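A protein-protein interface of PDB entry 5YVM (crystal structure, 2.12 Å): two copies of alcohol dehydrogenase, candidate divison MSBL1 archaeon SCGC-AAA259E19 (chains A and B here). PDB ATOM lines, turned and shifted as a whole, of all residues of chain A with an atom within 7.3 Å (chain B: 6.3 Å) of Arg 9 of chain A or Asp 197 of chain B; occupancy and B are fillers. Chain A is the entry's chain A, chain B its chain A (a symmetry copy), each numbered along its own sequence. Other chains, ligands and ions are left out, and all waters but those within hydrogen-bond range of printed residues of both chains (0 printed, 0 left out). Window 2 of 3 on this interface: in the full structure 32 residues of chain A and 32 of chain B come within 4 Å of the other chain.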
ATOM      1  N   HIS A   7     -28.174   9.999  10.781  1.00  0.00           N
ATOM      2  CA  HIS A   7     -28.859   9.899   9.491  1.00  0.00           C
ATOM      3  C   HIS A   7     -29.776   8.655   9.389  1.00  0.00           C
ATOM      4  O   HIS A   7     -29.409   7.560   9.820  1.00  0.00           O
ATOM      5  CB  HIS A   7     -27.825   9.895   8.356  1.00  0.00           C
ATOM      6  CG  HIS A   7     -28.347   9.355   7.061  1.00  0.00           C
ATOM      7  ND1 HIS A   7     -29.165  10.086   6.226  1.00  0.00           N
ATOM      8  CD2 HIS A   7     -28.168   8.156   6.455  1.00  0.00           C
ATOM      9  CE1 HIS A   7     -29.476   9.358   5.165  1.00  0.00           C
ATOM     10  NE2 HIS A   7     -28.881   8.184   5.278  1.00  0.00           N
ATOM     11  N   MET A   8     -30.969   8.842   8.812  1.00  0.00           N
ATOM     12  CA  MET A   8     -31.920   7.749   8.594  1.00  0.00           C
ATOM     13  C   MET A   8     -31.446   6.814   7.483  1.00  0.00           C
ATOM     14  O   MET A   8     -31.430   7.203   6.310  1.00  0.00           O
ATOM     15  CB  MET A   8     -33.295   8.313   8.235  1.00  0.00           C
ATOM     16  CG  MET A   8     -34.147   8.718   9.416  1.00  0.00           C
ATOM     17  SD  MET A   8     -35.861   9.149   9.007  1.00  0.00           S
ATOM     18  CE  MET A   8     -36.273   7.937   7.734  1.00  0.00           C
ATOM     19  N   ARG A   9     -31.103   5.577   7.839  1.00  0.00           N
ATOM     20  CA  ARG A   9     -30.675   4.612   6.837  1.00  0.00           C
ATOM     21  C   ARG A   9     -31.785   4.344   5.829  1.00  0.00           C
ATOM     22  O   ARG A   9     -32.970   4.280   6.169  1.00  0.00           O
ATOM     23  CB  ARG A   9     -30.253   3.305   7.492  1.00  0.00           C
ATOM     24  CG  ARG A   9     -29.059   3.430   8.385  1.00  0.00           C
ATOM     25  CD  ARG A   9     -27.739   3.283   7.646  1.00  0.00           C
ATOM     26  NE  ARG A   9     -26.658   3.404   8.617  1.00  0.00           N
ATOM     27  CZ  ARG A   9     -25.390   3.043   8.431  1.00  0.00           C
ATOM     28  NH1 ARG A   9     -24.987   2.517   7.281  1.00  0.00           N
ATOM     29  NH2 ARG A   9     -24.524   3.203   9.417  1.00  0.00           N
ATOM     30  N   MET A  10     -31.387   4.188   4.577  1.00  0.00           N
ATOM     31  CA  MET A  10     -32.323   3.907   3.505  1.00  0.00           C
ATOM     32  C   MET A  10     -32.321   2.404   3.251  1.00  0.00           C
ATOM     33  O   MET A  10     -31.256   1.778   3.182  1.00  0.00           O
ATOM     34  CB  MET A  10     -31.934   4.699   2.253  1.00  0.00           C
ATOM     35  CG  MET A  10     -32.813   4.478   1.040  1.00  0.00           C
ATOM     36  SD  MET A  10     -31.976   4.864  -0.521  1.00  0.00           S
ATOM     37  CE  MET A  10     -31.623   6.620  -0.344  1.00  0.00           C
ATOM     38  N   GLU A  11     -33.510   1.822   3.158  1.00  0.00           N
ATOM     39  CA  GLU A  11     -33.653   0.392   2.944  1.00  0.00           C
ATOM     40  C   GLU A  11     -34.868   0.138   2.065  1.00  0.00           C
ATOM     41  O   GLU A  11     -35.947   0.694   2.311  1.00  0.00           O
ATOM     42  CB  GLU A  11     -33.801  -0.356   4.271  1.00  0.00           C
ATOM     43  CG  GLU A  11     -33.475  -1.823   4.145  1.00  0.00           C
ATOM     44  CD  GLU A  11     -32.652  -2.365   5.315  1.00  0.00           C
ATOM     45  OE1 GLU A  11     -31.601  -1.755   5.688  1.00  0.00           O
ATOM     46  OE2 GLU A  11     -33.073  -3.414   5.869  1.00  0.00           O
ATOM     47  N   ASP A 227     -38.796   4.066   1.226  1.00  0.00           N
ATOM     48  CA  ASP A 227     -37.895   4.457   0.158  1.00  0.00           C
ATOM     49  C   ASP A 227     -38.197   3.637  -1.089  1.00  0.00           C
ATOM     50  O   ASP A 227     -38.403   2.421  -1.012  1.00  0.00           O
ATOM     51  CB  ASP A 227     -36.443   4.237   0.600  1.00  0.00           C
ATOM     52  CG  ASP A 227     -36.077   5.084   1.790  1.00  0.00           C
ATOM     53  OD1 ASP A 227     -36.413   6.289   1.763  1.00  0.00           O
ATOM     54  OD2 ASP A 227     -35.479   4.563   2.755  1.00  0.00           O
ATOM     55  N   LYS A 319     -40.395  14.314   5.504  1.00  0.00           N
ATOM     56  CA  LYS A 319     -40.078  13.464   4.356  1.00  0.00           C
ATOM     57  C   LYS A 319     -41.236  13.404   3.361  1.00  0.00           C
ATOM     58  O   LYS A 319     -41.017  13.449   2.144  1.00  0.00           O
ATOM     59  CB  LYS A 319     -39.709  12.054   4.831  1.00  0.00           C
ATOM     60  CG  LYS A 319     -39.258  11.088   3.731  1.00  0.00           C
ATOM     61  CD  LYS A 319     -39.272   9.675   4.324  1.00  0.00           C
ATOM     62  CE  LYS A 319     -39.084   8.565   3.298  1.00  0.00           C
ATOM     63  NZ  LYS A 319     -38.077   7.553   3.771  1.00  0.00           N
ATOM     64  N   GLY B  24     -29.747  -1.802   1.317  1.00  0.00           N
ATOM     65  CA  GLY B  24     -29.749  -1.386   2.703  1.00  0.00           C
ATOM     66  C   GLY B  24     -28.420  -1.754   3.316  1.00  0.00           C
ATOM     67  O   GLY B  24     -27.531  -2.264   2.653  1.00  0.00           O
ATOM     68  N   SER B  25     -28.299  -1.482   4.601  1.00  0.00           N
ATOM     69  CA  SER B  25     -27.082  -1.840   5.307  1.00  0.00           C
ATOM     70  C   SER B  25     -27.334  -3.117   6.098  1.00  0.00           C
ATOM     71  O   SER B  25     -28.372  -3.258   6.755  1.00  0.00           O
ATOM     72  CB  SER B  25     -26.603  -0.693   6.201  1.00  0.00           C
ATOM     73  OG  SER B  25     -27.613  -0.274   7.091  1.00  0.00           O
ATOM     74  N   GLY B  26     -26.399  -4.056   6.003  1.00  0.00           N
ATOM     75  CA  GLY B  26     -26.609  -5.370   6.565  1.00  0.00           C
ATOM     76  C   GLY B  26     -27.384  -6.319   5.683  1.00  0.00           C
ATOM     77  O   GLY B  26     -27.752  -7.403   6.145  1.00  0.00           O
ATOM     78  N   THR B  27     -27.656  -5.947   4.429  1.00  0.00           N
ATOM     79  CA  THR B  27     -28.401  -6.835   3.550  1.00  0.00           C
ATOM     80  C   THR B  27     -27.566  -8.006   3.054  1.00  0.00           C
ATOM     81  O   THR B  27     -28.106  -8.889   2.386  1.00  0.00           O
ATOM     82  CB  THR B  27     -28.973  -6.057   2.358  1.00  0.00           C
ATOM     83  OG1 THR B  27     -27.929  -5.322   1.700  1.00  0.00           O
ATOM     84  CG2 THR B  27     -30.066  -5.085   2.836  1.00  0.00           C
ATOM     85  N   PHE B  56     -16.308  -9.554   5.404  1.00  0.00           N
ATOM     86  CA  PHE B  56     -17.566  -9.859   4.725  1.00  0.00           C
ATOM     87  C   PHE B  56     -17.530 -11.224   4.060  1.00  0.00           C
ATOM     88  O   PHE B  56     -18.575 -11.866   3.909  1.00  0.00           O
ATOM     89  CB  PHE B  56     -17.890  -8.772   3.708  1.00  0.00           C
ATOM     90  CG  PHE B  56     -18.110  -7.453   4.340  1.00  0.00           C
ATOM     91  CD1 PHE B  56     -19.209  -7.251   5.163  1.00  0.00           C
ATOM     92  CD2 PHE B  56     -17.208  -6.427   4.155  1.00  0.00           C
ATOM     93  CE1 PHE B  56     -19.413  -6.038   5.775  1.00  0.00           C
ATOM     94  CE2 PHE B  56     -17.402  -5.207   4.760  1.00  0.00           C
ATOM     95  CZ  PHE B  56     -18.493  -5.008   5.578  1.00  0.00           C
ATOM     96  N   ASP B 195     -25.170  -3.604  -0.195  1.00  0.00           N
ATOM     97  CA  ASP B 195     -25.006  -3.497   1.253  1.00  0.00           C
ATOM     98  C   ASP B 195     -24.129  -2.292   1.554  1.00  0.00           C
ATOM     99  O   ASP B 195     -22.924  -2.321   1.284  1.00  0.00           O
ATOM    100  CB  ASP B 195     -24.396  -4.771   1.844  1.00  0.00           C
ATOM    101  CG  ASP B 195     -24.554  -4.846   3.364  1.00  0.00           C
ATOM    102  OD1 ASP B 195     -24.574  -3.777   4.010  1.00  0.00           O
ATOM    103  OD2 ASP B 195     -24.672  -5.968   3.924  1.00  0.00           O
ATOM    104  N   ILE B 196     -24.737  -1.254   2.139  1.00  0.00           N
ATOM    105  CA  ILE B 196     -24.017  -0.023   2.472  1.00  0.00           C
ATOM    106  C   ILE B 196     -22.818  -0.304   3.369  1.00  0.00           C
ATOM    107  O   ILE B 196     -21.798   0.399   3.294  1.00  0.00           O
ATOM    108  CB  ILE B 196     -24.987   0.988   3.126  1.00  0.00           C
ATOM    109  CG1 ILE B 196     -26.173   1.255   2.199  1.00  0.00           C
ATOM    110  CG2 ILE B 196     -24.275   2.282   3.480  1.00  0.00           C
ATOM    111  CD1 ILE B 196     -25.782   1.873   0.885  1.00  0.00           C
ATOM    112  N   ASP B 197     -22.904  -1.333   4.222  1.00  0.00           N
ATOM    113  CA  ASP B 197     -21.790  -1.638   5.119  1.00  0.00           C
ATOM    114  C   ASP B 197     -20.566  -2.137   4.372  1.00  0.00           C
ATOM    115  O   ASP B 197     -19.442  -1.981   4.852  1.00  0.00           O
ATOM    116  CB  ASP B 197     -22.216  -2.664   6.152  1.00  0.00           C
ATOM    117  CG  ASP B 197     -23.215  -2.108   7.110  1.00  0.00           C
ATOM    118  OD1 ASP B 197     -23.388  -0.869   7.075  1.00  0.00           O
ATOM    119  OD2 ASP B 197     -23.805  -2.886   7.895  1.00  0.00           O
ATOM    120  N   ILE B 198     -20.753  -2.748   3.211  1.00  0.00           N
ATOM    121  CA  ILE B 198     -19.603  -3.150   2.414  1.00  0.00           C
ATOM    122  C   ILE B 198     -19.053  -1.965   1.636  1.00  0.00           C
ATOM    123  O   ILE B 198     -17.838  -1.741   1.600  1.00  0.00           O
ATOM    124  CB  ILE B 198     -20.003  -4.315   1.494  1.00  0.00           C
ATOM    125  CG1 ILE B 198     -20.669  -5.410   2.325  1.00  0.00           C
ATOM    126  CG2 ILE B 198     -18.787  -4.864   0.780  1.00  0.00           C
ATOM    127  CD1 ILE B 198     -21.074  -6.611   1.514  1.00  0.00           C
ATOM    128  N   LEU B 199     -19.943  -1.172   1.027  1.00  0.00           N
ATOM    129  CA  LEU B 199     -19.516  -0.092   0.150  1.00  0.00           C
ATOM    130  C   LEU B 199     -18.823   1.023   0.914  1.00  0.00           C
ATOM    131  O   LEU B 199     -17.941   1.680   0.363  1.00  0.00           O
ATOM    132  CB  LEU B 199     -20.710   0.487  -0.597  1.00  0.00           C
ATOM    133  CG  LEU B 199     -21.576  -0.514  -1.324  1.00  0.00           C
ATOM    134  CD1 LEU B 199     -22.898   0.172  -1.650  1.00  0.00           C
ATOM    135  CD2 LEU B 199     -20.866  -0.915  -2.577  1.00  0.00           C
ATOM    136  N   LYS B 200     -19.231   1.269   2.162  1.00  0.00           N
ATOM    137  CA  LYS B 200     -18.635   2.326   2.963  1.00  0.00           C
ATOM    138  C   LYS B 200     -17.193   2.025   3.334  1.00  0.00           C
ATOM    139  O   LYS B 200     -16.512   2.912   3.852  1.00  0.00           O
ATOM    140  CB  LYS B 200     -19.453   2.560   4.237  1.00  0.00           C
ATOM    141  CG  LYS B 200     -19.186   1.540   5.317  1.00  0.00           C
ATOM    142  CD  LYS B 200     -19.873   1.914   6.621  1.00  0.00           C
ATOM    143  CE  LYS B 200     -19.339   1.065   7.768  1.00  0.00           C
ATOM    144  NZ  LYS B 200     -19.708   1.621   9.093  1.00  0.00           N
ATOM    145  N   GLU B 201     -16.711   0.811   3.070  1.00  0.00           N
ATOM    146  CA  GLU B 201     -15.306   0.471   3.256  1.00  0.00           C
ATOM    147  C   GLU B 201     -14.448   0.773   2.038  1.00  0.00           C
ATOM    148  O   GLU B 201     -13.230   0.620   2.121  1.00  0.00           O
ATOM    149  CB  GLU B 201     -15.156  -1.007   3.613  1.00  0.00           C
ATOM    150  CG  GLU B 201     -15.874  -1.379   4.880  1.00  0.00           C
ATOM    151  CD  GLU B 201     -15.445  -0.515   6.051  1.00  0.00           C
ATOM    152  OE1 GLU B 201     -14.259  -0.115   6.118  1.00  0.00           O
ATOM    153  OE2 GLU B 201     -16.301  -0.223   6.910  1.00  0.00           O
ATOM    154  N   ILE B 256     -22.743   8.330   5.382  1.00  0.00           N
ATOM    155  CA  ILE B 256     -23.634   7.248   4.972  1.00  0.00           C
ATOM    156  C   ILE B 256     -24.643   7.738   3.942  1.00  0.00           C
ATOM    157  O   ILE B 256     -24.979   7.014   2.996  1.00  0.00           O
ATOM    158  CB  ILE B 256     -24.336   6.631   6.198  1.00  0.00           C
ATOM    159  CG1 ILE B 256     -23.313   6.115   7.222  1.00  0.00           C
ATOM    160  CG2 ILE B 256     -25.298   5.524   5.755  1.00  0.00           C
ATOM    161  CD1 ILE B 256     -22.270   5.169   6.644  1.00  0.00           C
ATOM    162  N   GLU B 260     -25.083   6.020   0.383  1.00  0.00           N
ATOM    163  CA  GLU B 260     -26.380   5.537  -0.086  1.00  0.00           C
ATOM    164  C   GLU B 260     -26.719   6.103  -1.457  1.00  0.00           C
ATOM    165  O   GLU B 260     -27.181   5.375  -2.346  1.00  0.00           O
ATOM    166  CB  GLU B 260     -27.472   5.907   0.917  1.00  0.00           C
ATOM    167  CG  GLU B 260     -27.413   5.156   2.224  1.00  0.00           C
ATOM    168  CD  GLU B 260     -28.442   5.662   3.226  1.00  0.00           C
ATOM    169  OE1 GLU B 260     -28.999   6.766   3.022  1.00  0.00           O
ATOM    170  OE2 GLU B 260     -28.704   4.952   4.219  1.00  0.00           O
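No position is printed for both chains.
Of the 11 pairs that touch across the chains among the printed residues, none has its exchanged pair printed and touching as well.
His 7 of chain A touches Ile 256 of chain B (CD2 to CG2, 3.96 Å).
Ser 25 of chain B touches Arg 9 of chain A.
Arg 9 of chain A touches Ile 196 of chain B.
Ile 256 of chain B touches Arg 9 of chain A (CG2 to NH1, 3.4 Å).
CA of Arg 9 of chain A touches OE2 of Glu 260 of chain B (3.3 Å).
Gly 24 of chain B touches Met 10 of chain A (CA to O, 3.5 Å).
CA of Gly 24 of chain B touches OE1 of Glu 11 of chain A, at 3.5 Å.
Printed residues of chain B within 4 Å of Arg 9 of chain A: Ser 25 (3.6 Å), Ile 196 (3.9 Å), Asp 197 (3.8 Å), Ile 256 (3.4 Å) and Glu 260 (3.3 Å).
Printed residues of chain A within 4 Å of Ile 196 of chain B: Arg 9.
Printed residues of chain A within 4 Å of Ile 256 of chain B: His 7 and Arg 9.
Printed residues of chain A within 4 Å of Glu 260 of chain B: His 7, Arg 9 and Met 10.
The nearest printed residue of chain A that does not touch Asp 197 of chain B is Glu 11 of chain A (8.2 Å).
Along chain B the printed residues that touch a printed residue of chain A span positions 24 to 260.
Hydrophobic or aromatic side chains of chain A that line the printed part of chain B: His 7 and Met 10.
Among the printed residues, 11 pairs touch across the chains.
The guanidinium group (NH1) of Arg 9 of chain A lies within salt-bridge range of the side-chain carboxylate (OD1) of Asp 197 of chain B (3.8 Å).
The backbone NH of Met 10 of chain A is in hydrogen-bond range of the side-chain carboxylate of Glu 260 of chain B (2.8 Å).
The backbone NH (N) of Ser 25 of chain B is in hydrogen-bond range of the side-chain carboxylate (OE1) of Glu 11 of chain A (3.5 Å).
OE1 of Glu 260 of chain B sits at hydrogen-bond distance from NE2 of His 7 of chain A (2.7 Å).
The side-chain carboxylate (OD2) of Asp 197 of chain B lies within hydrogen-bond range of the backbone NH (N) of Gly 26 of chain B (3.4 Å).
The backbone carbonyl oxygen (O) of Gly 24 of chain B sits at hydrogen-bond distance from the backbone NH (N) of Ile 196 of chain B (3.0 Å).
N of Glu 11 of chain A is in hydrogen-bond range of OD2 of Asp 227 of chain A (3.4 Å).
The side-chain hydroxyl (OG1) of Thr 27 of chain B sits at hydrogen-bond distance from the backbone carbonyl oxygen (O) of Gly 24 of chain B, 3.2 Å away.
OD1 of Asp 195 of chain B sits at hydrogen-bond distance from N of Asp 197 of chain B (3.0 Å).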
